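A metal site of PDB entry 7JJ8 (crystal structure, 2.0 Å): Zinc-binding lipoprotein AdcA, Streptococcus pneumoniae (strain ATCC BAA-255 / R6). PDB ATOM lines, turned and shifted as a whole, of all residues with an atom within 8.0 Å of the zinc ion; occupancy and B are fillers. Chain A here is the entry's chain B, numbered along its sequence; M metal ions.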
ATOM      1  N   PHE A   9     -12.358   2.030  10.136  1.00  0.00           N
ATOM      2  CA  PHE A   9     -11.233   2.011  11.068  1.00  0.00           C
ATOM      3  C   PHE A   9     -10.362   0.797  10.802  1.00  0.00           C
ATOM      4  O   PHE A   9     -10.679  -0.037   9.949  1.00  0.00           O
ATOM      5  CB  PHE A   9     -11.693   2.089  12.537  1.00  0.00           C
ATOM      6  CG  PHE A   9     -12.515   0.916  13.010  1.00  0.00           C
ATOM      7  CD1 PHE A   9     -13.839   0.777  12.617  1.00  0.00           C
ATOM      8  CD2 PHE A   9     -11.975  -0.015  13.862  1.00  0.00           C
ATOM      9  CE1 PHE A   9     -14.603  -0.291  13.068  1.00  0.00           C
ATOM     10  CE2 PHE A   9     -12.715  -1.107  14.311  1.00  0.00           C
ATOM     11  CZ  PHE A   9     -14.035  -1.237  13.918  1.00  0.00           C
ATOM     12  N   GLU A  35     -10.656   7.941  18.225  1.00  0.00           N
ATOM     13  CA  GLU A  35     -11.490   6.842  18.717  1.00  0.00           C
ATOM     14  C   GLU A  35     -12.653   6.496  17.780  1.00  0.00           C
ATOM     15  O   GLU A  35     -13.590   7.295  17.618  1.00  0.00           O
ATOM     16  CB  GLU A  35     -11.997   7.184  20.126  1.00  0.00           C
ATOM     17  CG  GLU A  35     -13.045   6.211  20.645  1.00  0.00           C
ATOM     18  CD  GLU A  35     -12.606   4.751  20.497  1.00  0.00           C
ATOM     19  OE1 GLU A  35     -13.247   4.033  19.709  1.00  0.00           O
ATOM     20  OE2 GLU A  35     -11.623   4.310  21.136  1.00  0.00           O
ATOM     21  N   PRO A  36     -12.648   5.306  17.183  1.00  0.00           N
ATOM     22  CA  PRO A  36     -13.773   4.882  16.336  1.00  0.00           C
ATOM     23  C   PRO A  36     -15.105   4.786  17.057  1.00  0.00           C
ATOM     24  O   PRO A  36     -16.145   4.860  16.399  1.00  0.00           O
ATOM     25  CB  PRO A  36     -13.329   3.513  15.804  1.00  0.00           C
ATOM     26  CG  PRO A  36     -11.851   3.548  15.883  1.00  0.00           C
ATOM     27  CD  PRO A  36     -11.499   4.384  17.070  1.00  0.00           C
ATOM     28  N   HIS A  37     -15.132   4.565  18.376  1.00  0.00           N
ATOM     29  CA  HIS A  37     -16.410   4.520  19.077  1.00  0.00           C
ATOM     30  C   HIS A  37     -17.118   5.875  19.085  1.00  0.00           C
ATOM     31  O   HIS A  37     -18.350   5.922  19.150  1.00  0.00           O
ATOM     32  CB  HIS A  37     -16.261   4.022  20.514  1.00  0.00           C
ATOM     33  CG  HIS A  37     -16.045   2.543  20.616  1.00  0.00           C
ATOM     34  ND1 HIS A  37     -17.006   1.632  20.229  1.00  0.00           N
ATOM     35  CD2 HIS A  37     -15.025   1.812  21.139  1.00  0.00           C
ATOM     36  CE1 HIS A  37     -16.563   0.405  20.450  1.00  0.00           C
ATOM     37  NE2 HIS A  37     -15.365   0.485  21.007  1.00  0.00           N
ATOM     38  N   MET A  62     -21.083  -0.738  15.817  1.00  0.00           N
ATOM     39  CA  MET A  62     -19.801  -0.111  16.085  1.00  0.00           C
ATOM     40  C   MET A  62     -19.850   1.304  15.521  1.00  0.00           C
ATOM     41  O   MET A  62     -19.836   2.279  16.274  1.00  0.00           O
ATOM     42  CB  MET A  62     -18.664  -0.955  15.495  1.00  0.00           C
ATOM     43  CG  MET A  62     -17.328  -0.287  15.546  1.00  0.00           C
ATOM     44  SD  MET A  62     -16.673  -0.309  17.231  1.00  0.00           S
ATOM     45  CE  MET A  62     -16.492  -2.031  17.589  1.00  0.00           C
ATOM     46  N   ASP A 112     -22.654  -6.408  20.962  1.00  0.00           N
ATOM     47  CA  ASP A 112     -21.205  -6.222  21.070  1.00  0.00           C
ATOM     48  C   ASP A 112     -20.565  -6.340  19.690  1.00  0.00           C
ATOM     49  O   ASP A 112     -20.617  -7.420  19.082  1.00  0.00           O
ATOM     50  CB  ASP A 112     -20.652  -7.273  22.034  1.00  0.00           C
ATOM     51  CG  ASP A 112     -19.183  -7.098  22.328  1.00  0.00           C
ATOM     52  OD1 ASP A 112     -18.481  -6.380  21.569  1.00  0.00           O
ATOM     53  OD2 ASP A 112     -18.704  -7.714  23.320  1.00  0.00           O
ATOM     54  N   PRO A 113     -19.938  -5.288  19.177  1.00  0.00           N
ATOM     55  CA  PRO A 113     -19.406  -5.349  17.815  1.00  0.00           C
ATOM     56  C   PRO A 113     -18.006  -5.918  17.682  1.00  0.00           C
ATOM     57  O   PRO A 113     -17.576  -6.163  16.547  1.00  0.00           O
ATOM     58  CB  PRO A 113     -19.433  -3.868  17.407  1.00  0.00           C
ATOM     59  CG  PRO A 113     -19.136  -3.185  18.703  1.00  0.00           C
ATOM     60  CD  PRO A 113     -19.778  -3.960  19.786  1.00  0.00           C
ATOM     61  N   HIS A 114     -17.298  -6.191  18.800  1.00  0.00           N
ATOM     62  CA  HIS A 114     -15.848  -6.458  18.742  1.00  0.00           C
ATOM     63  C   HIS A 114     -15.430  -7.859  18.246  1.00  0.00           C
ATOM     64  O   HIS A 114     -14.575  -8.503  18.868  1.00  0.00           O
ATOM     65  CB  HIS A 114     -15.251  -6.242  20.139  1.00  0.00           C
ATOM     66  CG  HIS A 114     -15.344  -4.823  20.629  1.00  0.00           C
ATOM     67  ND1 HIS A 114     -16.318  -4.408  21.508  1.00  0.00           N
ATOM     68  CD2 HIS A 114     -14.520  -3.754  20.438  1.00  0.00           C
ATOM     69  CE1 HIS A 114     -16.139  -3.122  21.787  1.00  0.00           C
ATOM     70  NE2 HIS A 114     -15.045  -2.706  21.162  1.00  0.00           N
ATOM     71  N   TRP A 116     -13.586  -8.865  15.734  1.00  0.00           N
ATOM     72  CA  TRP A 116     -12.308  -9.035  15.043  1.00  0.00           C
ATOM     73  C   TRP A 116     -11.168  -9.392  15.999  1.00  0.00           C
ATOM     74  O   TRP A 116     -10.051  -9.659  15.520  1.00  0.00           O
ATOM     75  CB  TRP A 116     -11.914  -7.789  14.231  1.00  0.00           C
ATOM     76  CG  TRP A 116     -11.661  -6.580  15.096  1.00  0.00           C
ATOM     77  CD1 TRP A 116     -10.474  -6.199  15.652  1.00  0.00           C
ATOM     78  CD2 TRP A 116     -12.635  -5.641  15.560  1.00  0.00           C
ATOM     79  NE1 TRP A 116     -10.633  -5.063  16.402  1.00  0.00           N
ATOM     80  CE2 TRP A 116     -11.960  -4.703  16.380  1.00  0.00           C
ATOM     81  CE3 TRP A 116     -14.017  -5.477  15.356  1.00  0.00           C
ATOM     82  CZ2 TRP A 116     -12.600  -3.649  17.006  1.00  0.00           C
ATOM     83  CZ3 TRP A 116     -14.651  -4.415  15.960  1.00  0.00           C
ATOM     84  CH2 TRP A 116     -13.934  -3.522  16.789  1.00  0.00           C
ATOM     85  N   LEU A 117     -11.392  -9.371  17.306  1.00  0.00           N
ATOM     86  CA  LEU A 117     -10.359  -9.807  18.253  1.00  0.00           C
ATOM     87  C   LEU A 117     -10.305 -11.323  18.395  1.00  0.00           C
ATOM     88  O   LEU A 117      -9.473 -11.831  19.150  1.00  0.00           O
ATOM     89  CB  LEU A 117     -10.563  -9.150  19.637  1.00  0.00           C
ATOM     90  CG  LEU A 117     -10.205  -7.653  19.797  1.00  0.00           C
ATOM     91  CD1 LEU A 117      -8.816  -7.384  19.208  1.00  0.00           C
ATOM     92  CD2 LEU A 117     -11.239  -6.753  19.128  1.00  0.00           C
ATOM     93  N   HIS A 178     -10.685  -2.084  28.486  1.00  0.00           N
ATOM     94  CA  HIS A 178     -11.554  -1.929  27.316  1.00  0.00           C
ATOM     95  C   HIS A 178     -12.174  -3.285  26.987  1.00  0.00           C
ATOM     96  O   HIS A 178     -11.460  -4.233  26.658  1.00  0.00           O
ATOM     97  CB  HIS A 178     -10.772  -1.353  26.132  1.00  0.00           C
ATOM     98  CG  HIS A 178     -11.608  -0.999  24.936  1.00  0.00           C
ATOM     99  ND1 HIS A 178     -11.449   0.180  24.249  1.00  0.00           N
ATOM    100  CD2 HIS A 178     -12.569  -1.694  24.278  1.00  0.00           C
ATOM    101  CE1 HIS A 178     -12.303   0.225  23.236  1.00  0.00           C
ATOM    102  NE2 HIS A 178     -13.007  -0.896  23.244  1.00  0.00           N
ATOM    103  N   ALA A 179     -13.509  -3.364  27.053  1.00  0.00           N
ATOM    104  CA  ALA A 179     -14.234  -4.642  26.962  1.00  0.00           C
ATOM    105  C   ALA A 179     -14.401  -5.088  25.515  1.00  0.00           C
ATOM    106  O   ALA A 179     -15.508  -5.274  25.012  1.00  0.00           O
ATOM    107  CB  ALA A 179     -15.581  -4.515  27.658  1.00  0.00           C
ATOM    108  N   ALA A 180     -13.273  -5.280  24.842  1.00  0.00           N
ATOM    109  CA  ALA A 180     -13.264  -5.639  23.436  1.00  0.00           C
ATOM    110  C   ALA A 180     -13.034  -7.122  23.208  1.00  0.00           C
ATOM    111  O   ALA A 180     -12.855  -7.540  22.075  1.00  0.00           O
ATOM    112  CB  ALA A 180     -12.192  -4.836  22.691  1.00  0.00           C
ATOM    113  N   PHE A 181     -13.020  -7.920  24.276  1.00  0.00           N
ATOM    114  CA  PHE A 181     -12.503  -9.275  24.175  1.00  0.00           C
ATOM    115  C   PHE A 181     -13.525 -10.329  24.528  1.00  0.00           C
ATOM    116  O   PHE A 181     -13.152 -11.450  24.872  1.00  0.00           O
ATOM    117  CB  PHE A 181     -11.212  -9.359  25.012  1.00  0.00           C
ATOM    118  CG  PHE A 181     -10.200  -8.311  24.618  1.00  0.00           C
ATOM    119  CD1 PHE A 181      -9.380  -8.516  23.513  1.00  0.00           C
ATOM    120  CD2 PHE A 181     -10.163  -7.075  25.253  1.00  0.00           C
ATOM    121  CE1 PHE A 181      -8.484  -7.519  23.086  1.00  0.00           C
ATOM    122  CE2 PHE A 181      -9.272  -6.075  24.839  1.00  0.00           C
ATOM    123  CZ  PHE A 181      -8.442  -6.298  23.748  1.00  0.00           C
ATOM    124  N   GLU A 227      -5.874  -0.808  26.938  1.00  0.00           N
ATOM    125  CA  GLU A 227      -5.878  -0.773  25.475  1.00  0.00           C
ATOM    126  C   GLU A 227      -4.591  -0.177  24.925  1.00  0.00           C
ATOM    127  O   GLU A 227      -4.303  -0.370  23.743  1.00  0.00           O
ATOM    128  CB  GLU A 227      -7.067   0.026  24.983  1.00  0.00           C
ATOM    129  CG  GLU A 227      -7.081   1.472  25.429  1.00  0.00           C
ATOM    130  CD  GLU A 227      -8.360   2.150  24.988  1.00  0.00           C
ATOM    131  OE1 GLU A 227      -8.290   3.059  24.128  1.00  0.00           O
ATOM    132  OE2 GLU A 227      -9.436   1.747  25.480  1.00  0.00           O
ATOM    133  N   PRO A 251      -7.243  -3.453  21.472  1.00  0.00           N
ATOM    134  CA  PRO A 251      -8.477  -3.797  20.745  1.00  0.00           C
ATOM    135  C   PRO A 251      -8.407  -3.564  19.241  1.00  0.00           C
ATOM    136  O   PRO A 251      -9.391  -3.826  18.538  1.00  0.00           O
ATOM    137  CB  PRO A 251      -9.529  -2.874  21.375  1.00  0.00           C
ATOM    138  CG  PRO A 251      -8.724  -1.663  21.846  1.00  0.00           C
ATOM    139  CD  PRO A 251      -7.374  -2.220  22.275  1.00  0.00           C
ATOM    140  N   LEU A 252      -7.268  -3.071  18.755  1.00  0.00           N
ATOM    141  CA  LEU A 252      -7.021  -2.876  17.331  1.00  0.00           C
ATOM    142  C   LEU A 252      -8.075  -1.966  16.715  1.00  0.00           C
ATOM    143  O   LEU A 252      -8.524  -2.160  15.583  1.00  0.00           O
ATOM    144  CB  LEU A 252      -6.972  -4.214  16.602  1.00  0.00           C
ATOM    145  CG  LEU A 252      -5.594  -4.851  16.658  1.00  0.00           C
ATOM    146  CD1 LEU A 252      -5.671  -6.374  16.500  1.00  0.00           C
ATOM    147  CD2 LEU A 252      -4.690  -4.217  15.615  1.00  0.00           C
ATOM    148  N   GLU A 253      -8.454  -0.928  17.449  1.00  0.00           N
ATOM    149  CA  GLU A 253      -9.381   0.049  16.920  1.00  0.00           C
ATOM    150  C   GLU A 253      -8.670   1.227  16.260  1.00  0.00           C
ATOM    151  O   GLU A 253      -9.204   1.814  15.315  1.00  0.00           O
ATOM    152  CB  GLU A 253     -10.320   0.500  18.041  1.00  0.00           C
ATOM    153  CG  GLU A 253     -11.217  -0.667  18.478  1.00  0.00           C
ATOM    154  CD  GLU A 253     -12.077  -0.407  19.695  1.00  0.00           C
ATOM    155  OE1 GLU A 253     -12.017   0.703  20.264  1.00  0.00           O
ATOM    156  OE2 GLU A 253     -12.827  -1.335  20.094  1.00  0.00           O
HETATM  157 ZN    ZN M   1     -14.051  -1.005  21.479  1.00  0.00          ZN
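ND1 of His 114 sits at hydrogen-bond distance from OD1 of Asp 112, 2.9 Å away.
SD of Met 62 sits close to ND1 of His 37.
The side-chain carboxylate of Glu 227 is in hydrogen-bond range of a ring nitrogen (ND1) of His 178 (2.8 Å).
Of the 18 residues printed, 4 come within 4 Å of the zinc ion.
Along chain A the residues within 4 Å of the zinc ion span positions 37 to 253.
The nearest printed residue that does not touch the zinc ion is Ala 180 (4.4 Å).
The zinc ion is bound by the side-chain carboxylate of Glu 253 (1.9 Å), a ring nitrogen (NE2) of His 114 (2.0 Å), a ring nitrogen (NE2) of His 37 (2.0 Å) and a ring nitrogen (NE2) of His 178 (2.1 Å).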
